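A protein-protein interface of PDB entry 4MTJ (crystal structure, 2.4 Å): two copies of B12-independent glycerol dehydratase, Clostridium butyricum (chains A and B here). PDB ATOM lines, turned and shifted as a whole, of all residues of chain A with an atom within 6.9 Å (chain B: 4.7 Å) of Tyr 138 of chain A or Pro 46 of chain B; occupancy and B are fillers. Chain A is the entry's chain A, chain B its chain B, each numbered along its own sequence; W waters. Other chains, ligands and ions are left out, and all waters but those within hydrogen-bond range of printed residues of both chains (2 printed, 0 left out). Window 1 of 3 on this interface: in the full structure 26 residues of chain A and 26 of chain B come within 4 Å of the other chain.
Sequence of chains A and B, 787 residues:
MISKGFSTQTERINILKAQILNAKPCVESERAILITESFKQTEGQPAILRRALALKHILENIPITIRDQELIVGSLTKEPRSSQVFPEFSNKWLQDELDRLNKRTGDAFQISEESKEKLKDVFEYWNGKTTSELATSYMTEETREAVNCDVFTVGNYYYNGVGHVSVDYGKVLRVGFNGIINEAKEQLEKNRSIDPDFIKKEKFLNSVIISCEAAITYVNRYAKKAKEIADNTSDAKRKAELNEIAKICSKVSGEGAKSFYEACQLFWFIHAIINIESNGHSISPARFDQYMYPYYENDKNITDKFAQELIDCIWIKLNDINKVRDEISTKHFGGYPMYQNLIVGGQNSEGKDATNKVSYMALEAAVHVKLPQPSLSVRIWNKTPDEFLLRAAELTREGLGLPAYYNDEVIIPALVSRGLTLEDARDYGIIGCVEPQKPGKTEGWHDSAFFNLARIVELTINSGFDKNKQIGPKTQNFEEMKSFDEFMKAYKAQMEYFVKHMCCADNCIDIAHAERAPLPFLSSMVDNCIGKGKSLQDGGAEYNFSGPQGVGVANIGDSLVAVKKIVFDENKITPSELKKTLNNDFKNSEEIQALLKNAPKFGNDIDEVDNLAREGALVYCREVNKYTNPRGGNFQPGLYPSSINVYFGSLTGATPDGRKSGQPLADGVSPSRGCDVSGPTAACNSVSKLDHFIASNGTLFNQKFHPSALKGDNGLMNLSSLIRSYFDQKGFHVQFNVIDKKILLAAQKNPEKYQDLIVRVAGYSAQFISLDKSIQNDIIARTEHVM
The side-chain hydroxyl of Ser 137 of chain A is in hydrogen-bond range of the backbone carbonyl oxygen of Gly 44 of chain B, at 2.4 Å.
NZ of Lys 203 of chain B sits close to O of Tyr 138 of chain A.
The backbone carbonyl oxygen (O) of Glu 133 of chain A lies close to the backbone carbonyl oxygen (O) of Gly 44 of chain B (3.2 Å).
OG of Ser 137 of chain A lies within hydrogen-bond range of O of Glu 133 of chain A (3.0 Å).
SG of Cys 508 of chain A lies within hydrogen-bond range of O of Tyr 138 of chain A.
O of Met 139 of chain A is in hydrogen-bond range of NH2 of Arg 144 of chain A (3.0 Å).
The side-chain sulfur (SG) of Cys 508 of chain A sits at hydrogen-bond distance from the backbone NH (N) of Met 139 of chain A (3.6 Å).
O of Ser 137 of chain A sits at hydrogen-bond distance from NH2 of Arg 144 of chain A (3.4 Å).
The side-chain hydroxyl (OH) of Tyr 138 of chain A is in hydrogen-bond range of the side-chain carboxylate (OE1) of Glu 515 of chain A, 2.6 Å away.
Among the printed residues, pairs that only touch across the chains: Leu 134 of chain A with Gly 44 of chain B (3.4 Å), Leu 134 of chain A with Pro 46 of chain B (3.9 Å), Ser 137 of chain A with Gln 45 of chain B (3.3 Å), Ser 137 of chain A with Pro 46 of chain B (3.9 Å), Ser 137 of chain A with Lys 203 of chain B (3.6 Å), Tyr 138 of chain A with Pro 46 of chain B (3.8 Å), Tyr 138 of chain A with Ile 199 of chain B (3.8 Å), Met 139 of chain A with Lys 203 of chain B (3.7 Å), Asn 507 of chain A with Ile 199 of chain B (3.9 Å), Ile 511 of chain A with Ile 199 of chain B (3.8 Å) and Arg 516 of chain A with Gly 44 of chain B (3.9 Å).
Of the printed residues of chain B, Ser 137 of chain A touches Gly 44, Gln 45, Pro 46 and Lys 203.
Printed residues of chain B within 4 Å of Tyr 138 of chain A: Pro 46 (3.8 Å), Ile 199 (3.8 Å) and Lys 203 (3.1 Å).
Ile 509 of chain A touches none of the printed residues of chain B.
Printed residues of chain B within 4 Å of Ile 511 of chain A: Ile 199 (3.8 Å).
Glu 515 of chain A touches none of the printed residues of chain B.
Pro 46 of chain B touches three residues of chain A.
The nearest residue of chain B that does not touch Tyr 138 of chain A is Lys 200 of chain B (4.2 Å).
The nearest residue of chain A that does not touch Pro 46 of chain B is Glu 515 of chain A (4.5 Å).
The nearest printed residue of chain A that does not touch Gln 45 of chain B is Arg 516 of chain A (4.1 Å).
Hydrophobic or aromatic side chains of chain B within 4 Å of the printed part of chain A: Pro 46 and Ile 199.
Of the 17 printed residues of chain A, 8 touch a printed residue of chain B.
Among the printed residues, no Asp or Glu carboxylate lies within 4 Å of a Lys or Arg side-chain nitrogen of the other chain.
No position is printed for both chains.
Of the 14 pairs that touch across the chains among the printed residues, none has its exchanged pair printed and touching as well.
Water W1 lies within hydrogen-bond range of O of Gln 45 of chain B (2.6 Å) and NH2 of Arg 516 of chain A (3.4 Å).
Water W2 lies within hydrogen-bond range of OE2 of Glu 515 of chain A (2.6 Å) and N of Ala 47 of chain B (3.0 Å).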
ATOM      1  N   GLU A 133      19.228  11.966   3.888  1.00  0.00           N
ATOM      2  CA  GLU A 133      18.759  13.308   3.556  1.00  0.00           C
ATOM      3  C   GLU A 133      17.236  13.353   3.442  1.00  0.00           C
ATOM      4  O   GLU A 133      16.599  14.356   3.802  1.00  0.00           O
ATOM      5  CB  GLU A 133      19.445  13.843   2.290  1.00  0.00           C
ATOM      6  CG  GLU A 133      20.961  13.964   2.440  1.00  0.00           C
ATOM      7  CD  GLU A 133      21.725  13.876   1.113  1.00  0.00           C
ATOM      8  OE1 GLU A 133      22.320  14.904   0.713  1.00  0.00           O
ATOM      9  OE2 GLU A 133      21.738  12.793   0.477  1.00  0.00           O
ATOM     10  N   LEU A 134      16.636  12.273   2.958  1.00  0.00           N
ATOM     11  CA  LEU A 134      15.180  12.244   2.886  1.00  0.00           C
ATOM     12  C   LEU A 134      14.614  12.131   4.305  1.00  0.00           C
ATOM     13  O   LEU A 134      13.631  12.785   4.647  1.00  0.00           O
ATOM     14  CB  LEU A 134      14.689  11.103   1.993  1.00  0.00           C
ATOM     15  CG  LEU A 134      13.169  10.888   1.995  1.00  0.00           C
ATOM     16  CD1 LEU A 134      12.453  12.160   1.577  1.00  0.00           C
ATOM     17  CD2 LEU A 134      12.799   9.745   1.068  1.00  0.00           C
ATOM     18  N   ALA A 135      15.269  11.328   5.136  1.00  0.00           N
ATOM     19  CA  ALA A 135      14.818  11.098   6.509  1.00  0.00           C
ATOM     20  C   ALA A 135      14.752  12.390   7.307  1.00  0.00           C
ATOM     21  O   ALA A 135      13.774  12.636   8.023  1.00  0.00           O
ATOM     22  CB  ALA A 135      15.742  10.083   7.210  1.00  0.00           C
ATOM     23  N   THR A 136      15.808  13.198   7.183  1.00  0.00           N
ATOM     24  CA  THR A 136      15.880  14.510   7.823  1.00  0.00           C
ATOM     25  C   THR A 136      14.724  15.396   7.336  1.00  0.00           C
ATOM     26  O   THR A 136      14.108  16.114   8.124  1.00  0.00           O
ATOM     27  CB  THR A 136      17.230  15.218   7.521  1.00  0.00           C
ATOM     28  OG1 THR A 136      18.312  14.541   8.186  1.00  0.00           O
ATOM     29  CG2 THR A 136      17.193  16.675   7.954  1.00  0.00           C
ATOM     30  N   SER A 137      14.431  15.333   6.043  1.00  0.00           N
ATOM     31  CA  SER A 137      13.363  16.141   5.453  1.00  0.00           C
ATOM     32  C   SER A 137      12.007  15.801   6.067  1.00  0.00           C
ATOM     33  O   SER A 137      11.177  16.685   6.280  1.00  0.00           O
ATOM     34  CB  SER A 137      13.303  15.955   3.925  1.00  0.00           C
ATOM     35  OG  SER A 137      14.484  16.408   3.281  1.00  0.00           O
ATOM     36  N   TYR A 138      11.778  14.519   6.347  1.00  0.00           N
ATOM     37  CA  TYR A 138      10.510  14.088   6.956  1.00  0.00           C
ATOM     38  C   TYR A 138      10.326  14.485   8.436  1.00  0.00           C
ATOM     39  O   TYR A 138       9.201  14.675   8.896  1.00  0.00           O
ATOM     40  CB  TYR A 138      10.330  12.583   6.815  1.00  0.00           C
ATOM     41  CG  TYR A 138       9.703  12.149   5.513  1.00  0.00           C
ATOM     42  CD1 TYR A 138      10.342  11.243   4.679  1.00  0.00           C
ATOM     43  CD2 TYR A 138       8.457  12.634   5.125  1.00  0.00           C
ATOM     44  CE1 TYR A 138       9.759  10.843   3.486  1.00  0.00           C
ATOM     45  CE2 TYR A 138       7.862  12.230   3.938  1.00  0.00           C
ATOM     46  CZ  TYR A 138       8.519  11.337   3.121  1.00  0.00           C
ATOM     47  OH  TYR A 138       7.931  10.935   1.932  1.00  0.00           O
ATOM     48  N   MET A 139      11.424  14.590   9.180  1.00  0.00           N
ATOM     49  CA  MET A 139      11.358  14.987  10.585  1.00  0.00           C
ATOM     50  C   MET A 139      10.922  16.446  10.747  1.00  0.00           C
ATOM     51  O   MET A 139      11.257  17.288   9.921  1.00  0.00           O
ATOM     52  CB  MET A 139      12.717  14.794  11.266  1.00  0.00           C
ATOM     53  CG  MET A 139      13.263  13.393  11.194  1.00  0.00           C
ATOM     54  SD  MET A 139      14.866  13.262  11.992  1.00  0.00           S
ATOM     55  CE  MET A 139      15.450  11.747  11.238  1.00  0.00           C
ATOM     56  N   THR A 140      10.188  16.740  11.819  1.00  0.00           N
ATOM     57  CA  THR A 140       9.870  18.123  12.166  1.00  0.00           C
ATOM     58  C   THR A 140      11.108  18.809  12.718  1.00  0.00           C
ATOM     59  O   THR A 140      12.130  18.175  12.989  1.00  0.00           O
ATOM     60  CB  THR A 140       8.789  18.198  13.237  1.00  0.00           C
ATOM     61  OG1 THR A 140       9.291  17.637  14.466  1.00  0.00           O
ATOM     62  CG2 THR A 140       7.555  17.440  12.786  1.00  0.00           C
ATOM     63  N   ARG A 144      14.164  17.262  14.947  1.00  0.00           N
ATOM     64  CA  ARG A 144      15.583  17.435  14.628  1.00  0.00           C
ATOM     65  C   ARG A 144      16.370  17.980  15.825  1.00  0.00           C
ATOM     66  O   ARG A 144      17.534  17.618  16.037  1.00  0.00           O
ATOM     67  CB  ARG A 144      15.776  18.357  13.422  1.00  0.00           C
ATOM     68  CG  ARG A 144      15.123  17.878  12.154  1.00  0.00           C
ATOM     69  CD  ARG A 144      15.364  18.870  11.041  1.00  0.00           C
ATOM     70  NE  ARG A 144      14.639  18.481   9.843  1.00  0.00           N
ATOM     71  CZ  ARG A 144      13.733  19.237   9.240  1.00  0.00           C
ATOM     72  NH1 ARG A 144      13.446  20.447   9.717  1.00  0.00           N
ATOM     73  NH2 ARG A 144      13.122  18.786   8.150  1.00  0.00           N
ATOM     74  N   CYS A 504       9.403   8.838  16.686  1.00  0.00           N
ATOM     75  CA  CYS A 504       8.987   9.552  15.495  1.00  0.00           C
ATOM     76  C   CYS A 504      10.168   9.744  14.542  1.00  0.00           C
ATOM     77  O   CYS A 504      10.026   9.567  13.323  1.00  0.00           O
ATOM     78  CB  CYS A 504       8.318  10.879  15.867  1.00  0.00           C
ATOM     79  SG  CYS A 504       6.866  10.606  16.984  1.00  0.00           S
ATOM     80  N   ASN A 507      10.616   6.596  12.892  1.00  0.00           N
ATOM     81  CA  ASN A 507       9.590   6.432  11.861  1.00  0.00           C
ATOM     82  C   ASN A 507       9.890   7.201  10.566  1.00  0.00           C
ATOM     83  O   ASN A 507       9.614   6.710   9.473  1.00  0.00           O
ATOM     84  CB  ASN A 507       8.197   6.742  12.409  1.00  0.00           C
ATOM     85  CG  ASN A 507       7.692   5.649  13.367  1.00  0.00           C
ATOM     86  OD1 ASN A 507       8.088   4.482  13.256  1.00  0.00           O
ATOM     87  ND2 ASN A 507       6.811   6.023  14.299  1.00  0.00           N
ATOM     88  N   CYS A 508      10.489   8.384  10.698  1.00  0.00           N
ATOM     89  CA  CYS A 508      10.902   9.177   9.541  1.00  0.00           C
ATOM     90  C   CYS A 508      11.988   8.469   8.730  1.00  0.00           C
ATOM     91  O   CYS A 508      11.929   8.424   7.497  1.00  0.00           O
ATOM     92  CB  CYS A 508      11.353  10.578   9.978  1.00  0.00           C
ATOM     93  SG  CYS A 508       9.976  11.596  10.583  1.00  0.00           S
ATOM     94  N   ILE A 509      12.958   7.895   9.439  1.00  0.00           N
ATOM     95  CA  ILE A 509      13.977   7.043   8.835  1.00  0.00           C
ATOM     96  C   ILE A 509      13.389   5.780   8.179  1.00  0.00           C
ATOM     97  O   ILE A 509      13.843   5.370   7.114  1.00  0.00           O
ATOM     98  CB  ILE A 509      15.068   6.674   9.868  1.00  0.00           C
ATOM     99  CG1 ILE A 509      15.776   7.935  10.357  1.00  0.00           C
ATOM    100  CG2 ILE A 509      16.096   5.712   9.283  1.00  0.00           C
ATOM    101  CD1 ILE A 509      16.535   7.711  11.628  1.00  0.00           C
ATOM    102  N   ILE A 511      10.346   5.426   6.880  1.00  0.00           N
ATOM    103  CA  ILE A 511       9.743   5.895   5.646  1.00  0.00           C
ATOM    104  C   ILE A 511      10.792   6.149   4.577  1.00  0.00           C
ATOM    105  O   ILE A 511      10.608   5.760   3.419  1.00  0.00           O
ATOM    106  CB  ILE A 511       8.875   7.157   5.875  1.00  0.00           C
ATOM    107  CG1 ILE A 511       7.615   6.785   6.672  1.00  0.00           C
ATOM    108  CG2 ILE A 511       8.457   7.774   4.545  1.00  0.00           C
ATOM    109  CD1 ILE A 511       6.831   7.985   7.188  1.00  0.00           C
ATOM    110  N   ALA A 512      11.899   6.774   4.969  1.00  0.00           N
ATOM    111  CA  ALA A 512      12.955   7.101   4.016  1.00  0.00           C
ATOM    112  C   ALA A 512      13.491   5.852   3.336  1.00  0.00           C
ATOM    113  O   ALA A 512      13.630   5.819   2.109  1.00  0.00           O
ATOM    114  CB  ALA A 512      14.092   7.896   4.681  1.00  0.00           C
ATOM    115  N   GLU A 515      11.141   4.463   0.882  1.00  0.00           N
ATOM    116  CA  GLU A 515      10.944   5.359  -0.238  1.00  0.00           C
ATOM    117  C   GLU A 515      12.120   5.348  -1.224  1.00  0.00           C
ATOM    118  O   GLU A 515      11.919   5.544  -2.416  1.00  0.00           O
ATOM    119  CB  GLU A 515      10.652   6.769   0.280  1.00  0.00           C
ATOM    120  CG  GLU A 515      10.342   7.789  -0.801  1.00  0.00           C
ATOM    121  CD  GLU A 515       9.560   8.991  -0.269  1.00  0.00           C
ATOM    122  OE1 GLU A 515       8.885   8.847   0.785  1.00  0.00           O
ATOM    123  OE2 GLU A 515       9.618  10.073  -0.910  1.00  0.00           O
ATOM    124  N   ARG A 516      13.331   5.092  -0.729  1.00  0.00           N
ATOM    125  CA  ARG A 516      14.545   5.189  -1.554  1.00  0.00           C
ATOM    126  C   ARG A 516      15.457   3.957  -1.554  1.00  0.00           C
ATOM    127  O   ARG A 516      16.292   3.816  -2.442  1.00  0.00           O
ATOM    128  CB  ARG A 516      15.366   6.420  -1.171  1.00  0.00           C
ATOM    129  CG  ARG A 516      14.733   7.740  -1.568  1.00  0.00           C
ATOM    130  CD  ARG A 516      15.583   8.927  -1.133  1.00  0.00           C
ATOM    131  NE  ARG A 516      15.034  10.169  -1.669  1.00  0.00           N
ATOM    132  CZ  ARG A 516      15.646  11.350  -1.636  1.00  0.00           C
ATOM    133  NH1 ARG A 516      16.853  11.470  -1.084  1.00  0.00           N
ATOM    134  NH2 ARG A 516      15.054  12.411  -2.168  1.00  0.00           N
ATOM    135  N   GLY B  44      16.705  16.426  -1.744  1.00  0.00           N
ATOM    136  CA  GLY B  44      16.518  15.634  -0.534  1.00  0.00           C
ATOM    137  C   GLY B  44      15.143  15.728   0.111  1.00  0.00           C
ATOM    138  O   GLY B  44      14.925  15.240   1.218  1.00  0.00           O
ATOM    139  N   GLN B  45      14.210  16.343  -0.605  1.00  0.00           N
ATOM    140  CA  GLN B  45      12.885  16.666  -0.092  1.00  0.00           C
ATOM    141  C   GLN B  45      11.879  15.679  -0.700  1.00  0.00           C
ATOM    142  O   GLN B  45      12.096  15.178  -1.802  1.00  0.00           O
ATOM    143  CB  GLN B  45      12.579  18.108  -0.518  1.00  0.00           C
ATOM    144  CG  GLN B  45      11.799  18.963   0.435  1.00  0.00           C
ATOM    145  CD  GLN B  45      12.427  19.100   1.806  1.00  0.00           C
ATOM    146  OE1 GLN B  45      11.838  18.685   2.802  1.00  0.00           O
ATOM    147  NE2 GLN B  45      13.605  19.708   1.871  1.00  0.00           N
ATOM    148  N   PRO B  46      10.785  15.368   0.018  1.00  0.00           N
ATOM    149  CA  PRO B  46       9.744  14.530  -0.600  1.00  0.00           C
ATOM    150  C   PRO B  46       9.119  15.254  -1.801  1.00  0.00           C
ATOM    151  O   PRO B  46       9.154  16.487  -1.847  1.00  0.00           O
ATOM    152  CB  PRO B  46       8.688  14.382   0.496  1.00  0.00           C
ATOM    153  CG  PRO B  46       9.205  15.092   1.689  1.00  0.00           C
ATOM    154  CD  PRO B  46      10.383  15.906   1.327  1.00  0.00           C
ATOM    155  N   ALA B  47       8.544  14.510  -2.741  1.00  0.00           N
ATOM    156  CA  ALA B  47       7.976  15.102  -3.963  1.00  0.00           C
ATOM    157  C   ALA B  47       6.972  16.254  -3.738  1.00  0.00           C
ATOM    158  O   ALA B  47       6.970  17.240  -4.475  1.00  0.00           O
ATOM    159  CB  ALA B  47       7.354  14.020  -4.836  1.00  0.00           C
ATOM    160  N   ILE B  48       6.124  16.129  -2.723  1.00  0.00           N
ATOM    161  CA  ILE B  48       5.100  17.132  -2.478  1.00  0.00           C
ATOM    162  C   ILE B  48       5.742  18.462  -2.057  1.00  0.00           C
ATOM    163  O   ILE B  48       5.264  19.543  -2.428  1.00  0.00           O
ATOM    164  CB  ILE B  48       4.035  16.629  -1.428  1.00  0.00           C
ATOM    165  CG1 ILE B  48       2.827  17.573  -1.328  1.00  0.00           C
ATOM    166  CG2 ILE B  48       4.665  16.413  -0.059  1.00  0.00           C
ATOM    167  CD1 ILE B  48       1.925  17.548  -2.518  1.00  0.00           C
ATOM    168  N   LEU B  49       6.836  18.393  -1.304  1.00  0.00           N
ATOM    169  CA  LEU B  49       7.520  19.614  -0.899  1.00  0.00           C
ATOM    170  C   LEU B  49       8.323  20.218  -2.052  1.00  0.00           C
ATOM    171  O   LEU B  49       8.390  21.437  -2.190  1.00  0.00           O
ATOM    172  CB  LEU B  49       8.394  19.383   0.330  1.00  0.00           C
ATOM    173  CG  LEU B  49       7.674  19.646   1.652  1.00  0.00           C
ATOM    174  CD1 LEU B  49       8.421  19.040   2.825  1.00  0.00           C
ATOM    175  CD2 LEU B  49       7.468  21.141   1.842  1.00  0.00           C
ATOM    176  N   ARG B  50       8.913  19.367  -2.884  1.00  0.00           N
ATOM    177  CA  ARG B  50       9.601  19.847  -4.067  1.00  0.00           C
ATOM    178  C   ARG B  50       8.597  20.583  -4.950  1.00  0.00           C
ATOM    179  O   ARG B  50       8.909  21.634  -5.504  1.00  0.00           O
ATOM    180  CB  ARG B  50      10.273  18.698  -4.823  1.00  0.00           C
ATOM    181  CG  ARG B  50      11.268  17.892  -3.986  1.00  0.00           C
ATOM    182  CD  ARG B  50      11.961  16.862  -4.853  1.00  0.00           C
ATOM    183  NE  ARG B  50      13.063  17.447  -5.614  1.00  0.00           N
ATOM    184  CZ  ARG B  50      13.705  16.830  -6.604  1.00  0.00           C
ATOM    185  NH1 ARG B  50      13.343  15.611  -6.976  1.00  0.00           N
ATOM    186  NH2 ARG B  50      14.712  17.437  -7.231  1.00  0.00           N
ATOM    187  N   ILE B 199       2.779  11.698   9.425  1.00  0.00           N
ATOM    188  CA  ILE B 199       4.044  12.226   8.891  1.00  0.00           C
ATOM    189  C   ILE B 199       3.912  12.746   7.449  1.00  0.00           C
ATOM    190  O   ILE B 199       4.193  13.908   7.175  1.00  0.00           O
ATOM    191  CB  ILE B 199       5.191  11.183   8.992  1.00  0.00           C
ATOM    192  CG1 ILE B 199       5.615  11.006  10.452  1.00  0.00           C
ATOM    193  CG2 ILE B 199       6.392  11.600   8.137  1.00  0.00           C
ATOM    194  CD1 ILE B 199       6.403   9.748  10.730  1.00  0.00           C
ATOM    195  N   LYS B 200       3.455  11.890   6.544  1.00  0.00           N
ATOM    196  CA  LYS B 200       3.237  12.291   5.157  1.00  0.00           C
ATOM    197  C   LYS B 200       2.125  13.341   5.000  1.00  0.00           C
ATOM    198  O   LYS B 200       2.223  14.227   4.149  1.00  0.00           O
ATOM    199  CB  LYS B 200       2.924  11.069   4.291  1.00  0.00           C
ATOM    200  CG  LYS B 200       4.136  10.238   3.874  1.00  0.00           C
ATOM    201  CD  LYS B 200       3.671   8.960   3.157  1.00  0.00           C
ATOM    202  CE  LYS B 200       4.819   8.170   2.525  1.00  0.00           C
ATOM    203  NZ  LYS B 200       4.356   6.849   2.001  1.00  0.00           N
ATOM    204  N   LYS B 203       3.563  16.812   5.673  1.00  0.00           N
ATOM    205  CA  LYS B 203       4.295  17.383   4.560  1.00  0.00           C
ATOM    206  C   LYS B 203       3.319  17.891   3.495  1.00  0.00           C
ATOM    207  O   LYS B 203       3.541  18.946   2.910  1.00  0.00           O
ATOM    208  CB  LYS B 203       5.287  16.371   3.984  1.00  0.00           C
ATOM    209  CG  LYS B 203       6.311  15.884   4.998  1.00  0.00           C
ATOM    210  CD  LYS B 203       6.845  17.030   5.856  1.00  0.00           C
ATOM    211  CE  LYS B 203       7.601  16.519   7.064  1.00  0.00           C
ATOM    212  NZ  LYS B 203       8.162  17.613   7.915  1.00  0.00           N
HETATM  213  O   HOH W   1      11.925  13.063  -3.362  1.00  0.00           O
HETATM  214  O   HOH W   2       8.089  11.548  -2.484  1.00  0.00           O
